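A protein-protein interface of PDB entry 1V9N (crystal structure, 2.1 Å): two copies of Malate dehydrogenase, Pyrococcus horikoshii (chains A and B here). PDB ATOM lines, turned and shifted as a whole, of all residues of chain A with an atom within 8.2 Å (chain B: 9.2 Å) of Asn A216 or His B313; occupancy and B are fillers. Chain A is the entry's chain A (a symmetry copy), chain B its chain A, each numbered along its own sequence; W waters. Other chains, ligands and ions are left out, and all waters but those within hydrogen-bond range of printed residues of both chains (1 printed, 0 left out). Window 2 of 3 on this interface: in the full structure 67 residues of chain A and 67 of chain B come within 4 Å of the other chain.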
ATOM      1  N   ALA A 156       4.579 -29.722   4.821  1.00  0.00           N
ATOM      2  CA  ALA A 156       5.154 -28.426   5.160  1.00  0.00           C
ATOM      3  C   ALA A 156       4.767 -27.359   4.146  1.00  0.00           C
ATOM      4  O   ALA A 156       4.858 -27.573   2.936  1.00  0.00           O
ATOM      5  CB  ALA A 156       6.676 -28.529   5.242  1.00  0.00           C
ATOM      6  N   PRO A 157       4.329 -26.190   4.627  1.00  0.00           N
ATOM      7  CA  PRO A 157       3.943 -25.121   3.706  1.00  0.00           C
ATOM      8  C   PRO A 157       5.169 -24.646   2.932  1.00  0.00           C
ATOM      9  O   PRO A 157       6.304 -24.799   3.398  1.00  0.00           O
ATOM     10  CB  PRO A 157       3.387 -24.050   4.640  1.00  0.00           C
ATOM     11  CG  PRO A 157       4.205 -24.237   5.881  1.00  0.00           C
ATOM     12  CD  PRO A 157       4.227 -25.742   6.026  1.00  0.00           C
ATOM     13  N   THR A 158       4.934 -24.074   1.756  1.00  0.00           N
ATOM     14  CA  THR A 158       6.012 -23.587   0.913  1.00  0.00           C
ATOM     15  C   THR A 158       6.850 -22.544   1.642  1.00  0.00           C
ATOM     16  O   THR A 158       6.355 -21.477   2.011  1.00  0.00           O
ATOM     17  CB  THR A 158       5.458 -22.979  -0.388  1.00  0.00           C
ATOM     18  OG1 THR A 158       4.685 -23.969  -1.080  1.00  0.00           O
ATOM     19  CG2 THR A 158       6.598 -22.513  -1.292  1.00  0.00           C
ATOM     20  N   GLY A 159       8.124 -22.866   1.844  1.00  0.00           N
ATOM     21  CA  GLY A 159       9.017 -21.955   2.532  1.00  0.00           C
ATOM     22  C   GLY A 159       9.222 -22.335   3.984  1.00  0.00           C
ATOM     23  O   GLY A 159       9.947 -21.653   4.714  1.00  0.00           O
ATOM     24  N   GLY A 160       8.590 -23.428   4.403  1.00  0.00           N
ATOM     25  CA  GLY A 160       8.701 -23.877   5.779  1.00  0.00           C
ATOM     26  C   GLY A 160       9.198 -25.301   5.895  1.00  0.00           C
ATOM     27  O   GLY A 160       9.449 -25.958   4.885  1.00  0.00           O
ATOM     28  N   ILE A 161       9.330 -25.787   7.126  1.00  0.00           N
ATOM     29  CA  ILE A 161       9.822 -27.140   7.355  1.00  0.00           C
ATOM     30  C   ILE A 161       8.997 -27.962   8.343  1.00  0.00           C
ATOM     31  O   ILE A 161       9.254 -29.149   8.528  1.00  0.00           O
ATOM     32  CB  ILE A 161      11.292 -27.108   7.846  1.00  0.00           C
ATOM     33  CG1 ILE A 161      11.391 -26.336   9.162  1.00  0.00           C
ATOM     34  CG2 ILE A 161      12.168 -26.438   6.803  1.00  0.00           C
ATOM     35  CD1 ILE A 161      12.811 -26.206   9.692  1.00  0.00           C
ATOM     36  N   GLU A 162       8.012 -27.335   8.977  1.00  0.00           N
ATOM     37  CA  GLU A 162       7.164 -28.032   9.945  1.00  0.00           C
ATOM     38  C   GLU A 162       6.013 -28.787   9.293  1.00  0.00           C
ATOM     39  O   GLU A 162       5.528 -28.392   8.236  1.00  0.00           O
ATOM     40  CB  GLU A 162       6.538 -27.048  10.926  1.00  0.00           C
ATOM     41  CG  GLU A 162       7.460 -26.400  11.916  1.00  0.00           C
ATOM     42  CD  GLU A 162       6.672 -25.595  12.932  1.00  0.00           C
ATOM     43  OE1 GLU A 162       5.814 -26.192  13.620  1.00  0.00           O
ATOM     44  OE2 GLU A 162       6.897 -24.374  13.039  1.00  0.00           O
ATOM     45  N   ASN A 212      10.183 -34.988  -0.195  1.00  0.00           N
ATOM     46  CA  ASN A 212      11.469 -34.925   0.461  1.00  0.00           C
ATOM     47  C   ASN A 212      11.672 -33.736   1.369  1.00  0.00           C
ATOM     48  O   ASN A 212      11.933 -32.624   0.919  1.00  0.00           O
ATOM     49  N   ARG A 213      11.529 -33.980   2.661  1.00  0.00           N
ATOM     50  CA  ARG A 213      11.745 -32.949   3.655  1.00  0.00           C
ATOM     51  C   ARG A 213      12.437 -33.739   4.744  1.00  0.00           C
ATOM     52  O   ARG A 213      11.826 -34.629   5.328  1.00  0.00           O
ATOM     53  N   GLU A 214      13.704 -33.449   5.014  1.00  0.00           N
ATOM     54  CA  GLU A 214      14.406 -34.214   6.028  1.00  0.00           C
ATOM     55  C   GLU A 214      14.409 -33.585   7.401  1.00  0.00           C
ATOM     56  O   GLU A 214      13.361 -33.395   8.016  1.00  0.00           O
ATOM     57  N   GLY A 215      15.606 -33.280   7.887  1.00  0.00           N
ATOM     58  CA  GLY A 215      15.738 -32.650   9.185  1.00  0.00           C
ATOM     59  C   GLY A 215      15.566 -31.163   8.977  1.00  0.00           C
ATOM     60  O   GLY A 215      14.817 -30.505   9.696  1.00  0.00           O
ATOM     61  N   ASN A 216      16.265 -30.640   7.974  1.00  0.00           N
ATOM     62  CA  ASN A 216      16.180 -29.229   7.654  1.00  0.00           C
ATOM     63  C   ASN A 216      15.514 -29.048   6.304  1.00  0.00           C
ATOM     64  O   ASN A 216      15.107 -27.943   5.940  1.00  0.00           O
ATOM     65  N   ILE A 217      15.404 -30.143   5.556  1.00  0.00           N
ATOM     66  CA  ILE A 217      14.779 -30.088   4.247  1.00  0.00           C
ATOM     67  C   ILE A 217      15.641 -30.656   3.136  1.00  0.00           C
ATOM     68  O   ILE A 217      16.405 -29.928   2.506  1.00  0.00           O
ATOM     69  N   THR A 218      15.517 -31.957   2.889  1.00  0.00           N
ATOM     70  CA  THR A 218      16.303 -32.579   1.840  1.00  0.00           C
ATOM     71  C   THR A 218      15.618 -33.753   1.168  1.00  0.00           C
ATOM     72  O   THR A 218      15.159 -33.647   0.031  1.00  0.00           O
ATOM     73  N   THR A 219      15.556 -34.880   1.872  1.00  0.00           N
ATOM     74  CA  THR A 219      14.929 -36.072   1.328  1.00  0.00           C
ATOM     75  C   THR A 219      15.275 -37.290   2.162  1.00  0.00           C
ATOM     76  O   THR A 219      14.860 -37.395   3.319  1.00  0.00           O
ATOM     77  N   GLU A 223      14.219 -40.322   7.214  1.00  0.00           N
ATOM     78  CA  GLU A 223      14.268 -39.074   7.953  1.00  0.00           C
ATOM     79  C   GLU A 223      12.916 -38.389   7.953  1.00  0.00           C
ATOM     80  O   GLU A 223      12.726 -37.362   8.607  1.00  0.00           O
ATOM     81  N   ASN A 226      11.237 -39.362  11.206  1.00  0.00           N
ATOM     82  CA  ASN A 226      11.968 -38.691  12.266  1.00  0.00           C
ATOM     83  C   ASN A 226      11.959 -37.183  12.106  1.00  0.00           C
ATOM     84  O   ASN A 226      12.956 -36.590  11.694  1.00  0.00           O
ATOM     85  N   GLY A 227      10.826 -36.564  12.427  1.00  0.00           N
ATOM     86  CA  GLY A 227      10.715 -35.120  12.319  1.00  0.00           C
ATOM     87  C   GLY A 227      10.696 -34.599  10.894  1.00  0.00           C
ATOM     88  O   GLY A 227      10.865 -33.402  10.663  1.00  0.00           O
ATOM     89  N   GLY A 228      10.496 -35.497   9.933  1.00  0.00           N
ATOM     90  CA  GLY A 228      10.454 -35.088   8.540  1.00  0.00           C
ATOM     91  C   GLY A 228       9.064 -34.623   8.142  1.00  0.00           C
ATOM     92  O   GLY A 228       8.149 -34.606   8.966  1.00  0.00           O
ATOM     93  N   LEU A 231       6.126 -33.191   0.986  1.00  0.00           N
ATOM     94  CA  LEU A 231       6.154 -31.999   0.149  1.00  0.00           C
ATOM     95  C   LEU A 231       4.802 -31.857  -0.563  1.00  0.00           C
ATOM     96  O   LEU A 231       4.164 -32.850  -0.899  1.00  0.00           O
ATOM     97  CB  LEU A 231       7.286 -32.123  -0.882  1.00  0.00           C
ATOM     98  CG  LEU A 231       8.399 -31.063  -0.928  1.00  0.00           C
ATOM     99  CD1 LEU A 231       8.939 -30.776   0.462  1.00  0.00           C
ATOM    100  CD2 LEU A 231       9.512 -31.553  -1.846  1.00  0.00           C
ATOM    101  N   PHE A 236       9.387 -29.004  -3.806  1.00  0.00           N
ATOM    102  CA  PHE A 236      10.082 -28.262  -2.765  1.00  0.00           C
ATOM    103  C   PHE A 236       9.983 -26.744  -2.761  1.00  0.00           C
ATOM    104  O   PHE A 236       9.909 -26.145  -1.699  1.00  0.00           O
ATOM    105  CB  PHE A 236      11.565 -28.670  -2.765  1.00  0.00           C
ATOM    106  CG  PHE A 236      12.427 -27.867  -1.826  1.00  0.00           C
ATOM    107  CD1 PHE A 236      12.860 -26.589  -2.169  1.00  0.00           C
ATOM    108  CD2 PHE A 236      12.799 -28.387  -0.591  1.00  0.00           C
ATOM    109  CE1 PHE A 236      13.650 -25.841  -1.297  1.00  0.00           C
ATOM    110  CE2 PHE A 236      13.590 -27.645   0.288  1.00  0.00           C
ATOM    111  CZ  PHE A 236      14.014 -26.369  -0.067  1.00  0.00           C
ATOM    112  N   ILE B 307       0.349 -20.494  10.225  1.00  0.00           N
ATOM    113  CA  ILE B 307       1.090 -21.075   9.109  1.00  0.00           C
ATOM    114  C   ILE B 307       2.300 -20.190   8.799  1.00  0.00           C
ATOM    115  O   ILE B 307       3.416 -20.681   8.629  1.00  0.00           O
ATOM    116  CB  ILE B 307       0.221 -21.177   7.832  1.00  0.00           C
ATOM    117  CG1 ILE B 307      -0.905 -22.195   8.039  1.00  0.00           C
ATOM    118  CG2 ILE B 307       1.087 -21.580   6.640  1.00  0.00           C
ATOM    119  CD1 ILE B 307      -1.803 -22.361   6.819  1.00  0.00           C
ATOM    120  N   LYS B 308       2.068 -18.884   8.720  1.00  0.00           N
ATOM    121  CA  LYS B 308       3.139 -17.942   8.418  1.00  0.00           C
ATOM    122  C   LYS B 308       4.212 -17.977   9.495  1.00  0.00           C
ATOM    123  O   LYS B 308       5.406 -17.933   9.195  1.00  0.00           O
ATOM    124  CB  LYS B 308       2.576 -16.522   8.287  1.00  0.00           C
ATOM    125  CG  LYS B 308       1.633 -16.344   7.103  1.00  0.00           C
ATOM    126  CD  LYS B 308       0.992 -14.968   7.075  1.00  0.00           C
ATOM    127  CE  LYS B 308       2.013 -13.868   6.833  1.00  0.00           C
ATOM    128  NZ  LYS B 308       2.732 -14.022   5.535  1.00  0.00           N
ATOM    129  N   SER B 310       5.094 -20.438  11.284  1.00  0.00           N
ATOM    130  CA  SER B 310       5.722 -21.746  11.451  1.00  0.00           C
ATOM    131  C   SER B 310       7.201 -21.684  11.073  1.00  0.00           C
ATOM    132  O   SER B 310       7.632 -20.790  10.346  1.00  0.00           O
ATOM    133  CB  SER B 310       5.001 -22.813  10.614  1.00  0.00           C
ATOM    134  OG  SER B 310       5.206 -22.633   9.225  1.00  0.00           O
ATOM    135  N   ARG B 311       7.971 -22.642  11.574  1.00  0.00           N
ATOM    136  CA  ARG B 311       9.413 -22.711  11.335  1.00  0.00           C
ATOM    137  C   ARG B 311       9.825 -22.511   9.877  1.00  0.00           C
ATOM    138  O   ARG B 311       9.568 -23.368   9.029  1.00  0.00           O
ATOM    139  CB  ARG B 311       9.937 -24.053  11.837  1.00  0.00           C
ATOM    140  CG  ARG B 311      11.409 -24.086  12.187  1.00  0.00           C
ATOM    141  CD  ARG B 311      11.720 -25.425  12.821  1.00  0.00           C
ATOM    142  NE  ARG B 311      10.744 -25.725  13.866  1.00  0.00           N
ATOM    143  CZ  ARG B 311      10.341 -26.949  14.187  1.00  0.00           C
ATOM    144  NH1 ARG B 311      10.830 -28.003  13.546  1.00  0.00           N
ATOM    145  NH2 ARG B 311       9.438 -27.118  15.146  1.00  0.00           N
ATOM    146  N   LYS B 312      10.473 -21.382   9.599  1.00  0.00           N
ATOM    147  CA  LYS B 312      10.936 -21.055   8.252  1.00  0.00           C
ATOM    148  C   LYS B 312      12.139 -21.895   7.833  1.00  0.00           C
ATOM    149  O   LYS B 312      12.989 -22.236   8.656  1.00  0.00           O
ATOM    150  CB  LYS B 312      11.322 -19.574   8.164  1.00  0.00           C
ATOM    151  CG  LYS B 312      10.397 -18.721   7.312  1.00  0.00           C
ATOM    152  CD  LYS B 312       9.586 -17.760   8.164  1.00  0.00           C
ATOM    153  CE  LYS B 312       8.668 -18.501   9.117  1.00  0.00           C
ATOM    154  NZ  LYS B 312       7.939 -17.579  10.029  1.00  0.00           N
ATOM    155  N   HIS B 313      12.207 -22.221   6.547  1.00  0.00           N
ATOM    156  CA  HIS B 313      13.312 -23.004   6.002  1.00  0.00           C
ATOM    157  C   HIS B 313      14.526 -22.077   5.927  1.00  0.00           C
ATOM    158  O   HIS B 313      14.383 -20.889   5.636  1.00  0.00           O
ATOM    159  CB  HIS B 313      12.938 -23.515   4.604  1.00  0.00           C
ATOM    160  CG  HIS B 313      13.993 -24.362   3.960  1.00  0.00           C
ATOM    161  ND1 HIS B 313      15.188 -23.845   3.503  1.00  0.00           N
ATOM    162  CD2 HIS B 313      14.031 -25.688   3.694  1.00  0.00           C
ATOM    163  CE1 HIS B 313      15.914 -24.817   2.981  1.00  0.00           C
ATOM    164  NE2 HIS B 313      15.235 -25.947   3.084  1.00  0.00           N
ATOM    165  N   PRO B 314      15.733 -22.603   6.199  1.00  0.00           N
ATOM    166  CA  PRO B 314      16.922 -21.747   6.142  1.00  0.00           C
ATOM    167  C   PRO B 314      17.027 -20.929   4.848  1.00  0.00           C
ATOM    168  O   PRO B 314      17.317 -19.739   4.890  1.00  0.00           O
ATOM    169  CB  PRO B 314      18.077 -22.741   6.320  1.00  0.00           C
ATOM    170  CG  PRO B 314      17.504 -24.038   5.822  1.00  0.00           C
ATOM    171  CD  PRO B 314      16.112 -24.012   6.397  1.00  0.00           C
ATOM    172  N   GLU B 315      16.763 -21.560   3.713  1.00  0.00           N
ATOM    173  CA  GLU B 315      16.858 -20.898   2.428  1.00  0.00           C
ATOM    174  C   GLU B 315      15.817 -19.820   2.135  1.00  0.00           C
ATOM    175  O   GLU B 315      16.027 -18.896   1.316  1.00  0.00           O
ATOM    176  CB  GLU B 315      16.788 -21.938   1.302  1.00  0.00           C
ATOM    177  CG  GLU B 315      18.033 -22.820   1.172  1.00  0.00           C
ATOM    178  CD  GLU B 315      19.261 -22.021   0.793  1.00  0.00           C
ATOM    179  OE1 GLU B 315      19.243 -21.376  -0.278  1.00  0.00           O
ATOM    180  OE2 GLU B 315      20.238 -22.034   1.572  1.00  0.00           O
ATOM    181  N   PHE B 316      14.682 -19.971   2.829  1.00  0.00           N
ATOM    182  CA  PHE B 316      13.530 -19.091   2.682  1.00  0.00           C
ATOM    183  C   PHE B 316      13.419 -17.922   3.654  1.00  0.00           C
ATOM    184  O   PHE B 316      13.833 -18.017   4.788  1.00  0.00           O
ATOM    185  CB  PHE B 316      12.272 -19.974   2.705  1.00  0.00           C
ATOM    186  CG  PHE B 316      12.146 -20.830   1.475  1.00  0.00           C
ATOM    187  CD1 PHE B 316      12.118 -20.204   0.236  1.00  0.00           C
ATOM    188  CD2 PHE B 316      11.946 -22.210   1.528  1.00  0.00           C
ATOM    189  CE1 PHE B 316      11.871 -20.912  -0.922  1.00  0.00           C
ATOM    190  CE2 PHE B 316      11.693 -22.940   0.344  1.00  0.00           C
ATOM    191  CZ  PHE B 316      11.650 -22.274  -0.879  1.00  0.00           C
ATOM    192  N   GLU B 317      12.863 -16.802   3.234  1.00  0.00           N
ATOM    193  CA  GLU B 317      12.808 -15.662   4.141  1.00  0.00           C
ATOM    194  C   GLU B 317      11.487 -15.636   4.866  1.00  0.00           C
ATOM    195  O   GLU B 317      11.366 -15.298   6.064  1.00  0.00           O
ATOM    196  CB  GLU B 317      12.959 -14.395   3.291  1.00  0.00           C
ATOM    197  CG  GLU B 317      12.089 -13.184   3.559  1.00  0.00           C
ATOM    198  CD  GLU B 317      12.253 -12.683   4.962  1.00  0.00           C
ATOM    199  OE1 GLU B 317      13.318 -12.957   5.556  1.00  0.00           O
ATOM    200  OE2 GLU B 317      11.325 -12.011   5.460  1.00  0.00           O
ATOM    201  N   ARG B 318      10.481 -16.047   4.118  1.00  0.00           N
ATOM    202  CA  ARG B 318       9.144 -15.887   4.627  1.00  0.00           C
ATOM    203  C   ARG B 318       8.210 -16.923   4.069  1.00  0.00           C
ATOM    204  O   ARG B 318       8.447 -17.463   2.996  1.00  0.00           O
ATOM    205  CB  ARG B 318       8.792 -14.468   4.199  1.00  0.00           C
ATOM    206  CG  ARG B 318       7.402 -14.048   4.291  1.00  0.00           C
ATOM    207  CD  ARG B 318       7.364 -12.662   3.702  1.00  0.00           C
ATOM    208  NE  ARG B 318       6.082 -12.044   3.979  1.00  0.00           N
ATOM    209  CZ  ARG B 318       5.820 -10.758   3.793  1.00  0.00           C
ATOM    210  NH1 ARG B 318       6.762  -9.956   3.326  1.00  0.00           N
ATOM    211  NH2 ARG B 318       4.620 -10.271   4.079  1.00  0.00           N
ATOM    212  N   ILE B 319       7.169 -17.212   4.827  1.00  0.00           N
ATOM    213  CA  ILE B 319       6.143 -18.150   4.388  1.00  0.00           C
ATOM    214  C   ILE B 319       4.977 -17.236   4.036  1.00  0.00           C
ATOM    215  O   ILE B 319       4.485 -16.494   4.888  1.00  0.00           O
ATOM    216  CB  ILE B 319       5.721 -19.115   5.519  1.00  0.00           C
ATOM    217  CG1 ILE B 319       6.879 -20.060   5.852  1.00  0.00           C
ATOM    218  CG2 ILE B 319       4.490 -19.904   5.093  1.00  0.00           C
ATOM    219  CD1 ILE B 319       6.622 -20.972   7.035  1.00  0.00           C
HETATM  220  O   HOH W   1       6.800 -24.707   8.419  1.00  0.00           O
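O of Ser B310 sits close to NZ of Lys B312, at 3.2 Å.
O of Lys B308 lies within hydrogen-bond range of NZ of Lys B312.
The side-chain amino group (NZ) of Lys B308 sits at hydrogen-bond distance from the backbone carbonyl oxygen (O) of Ile B319 (3.1 Å).
The side-chain hydroxyl of Ser B310 is in hydrogen-bond range of the backbone carbonyl oxygen of Ile B307.
A ring nitrogen (ND1) of His B313 lies within hydrogen-bond range of the backbone NH of Glu B315, 2.8 Å away.
Water W1 lies within hydrogen-bond range of OG of Ser B310 (2.7 Å), N of Glu A162 (2.9 Å), N of Ile A161 (3.0 Å) and O of Arg B311 (3.1 Å).
N of Arg B311 is in hydrogen-bond range of OE2 of Glu A162.
O of Asn A216 lies close to NE2 of His B313 (3.5 Å).
The backbone NH (N) of Ile A161 lies within hydrogen-bond range of the backbone carbonyl oxygen (O) of Arg B311.
N of His B313 is in hydrogen-bond range of O of Gly A159 (3.0 Å).
Of chain B, only Arg B311 (3.4 Å), His B313 (3.95 Å) and Ile B319 (3.8 Å) come within 4 Å of Gly A160.
No residue of chain B comes within 4 Å of Glu A214.
No residue of chain B comes within 4 Å of Gly A215.
Asn A216 touches one residue of chain B.
Of the printed residues of chain B, Phe A236 touches His B313 (3.4 Å) and Phe B316 (3.9 Å).
Printed residues of chain A within 4 Å of Lys B312: Gly A159.
His B313 touches just these residues of chain A: Gly A159, Gly A160, Ile A161, Asn A216 and Phe A236.
No residue of chain A comes within 4 Å of Pro B314.
Printed residues of chain A within 4 Å of Phe B316: Gly A159 and Phe A236.
The nearest residue of chain B that does not touch Asn A216 is Pro B314 (4.1 Å).
The nearest residue of chain A that does not touch His B313 is Ile A217 (4.2 Å).
Printed residues of chain B that touch a printed residue of chain A: Ile B307, Ser B310, Arg B311, Lys B312, His B313, Phe B316 and Ile B319.
Hydrophobic or aromatic side chains of chain B that line the printed part of chain A: Ile B307, His B313, Phe B316 and Ile B319.
Along chain B the printed residues that touch a printed residue of chain A span positions 307 to 319.
Of the 21 printed residues of chain A, 8 touch a printed residue of chain B.
Hydrophobic or aromatic side chains of chain A within 4 Å of the printed part of chain B: Pro A157, Ile A161 and Phe A236.
Among the printed residues, 17 pairs touch across the chains.
Among the printed residues, no Asp or Glu carboxylate lies within 4 Å of a Lys or Arg side-chain nitrogen of the other chain.
Pro A157 touches Ser B310 (CG to OG, 3.8 Å).
O of Gly A159 touches CA of Lys B312 (3.7 Å).
Gly A159 touches Phe B316.
O of Gly A159 touches CG1 of Ile B319, at 3.6 Å.
CA of Gly A160 touches O of Arg B311, 3.4 Å away.
CA of Gly A160 touches CD1 of Ile B319, 3.8 Å away.
Ile A161 touches His B313.
Glu A162 touches Ser B310 (OE2 to CA, 3.3 Å).
CZ of Phe A236 touches NE2 of His B313, 3.4 Å away.
Phe A236 touches Phe B316 (CE1 to CE2, 3.9 Å).
No position is printed for both chains.
Of the 17 pairs that touch across the chains among the printed residues, none has its exchanged pair printed and touching as well.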
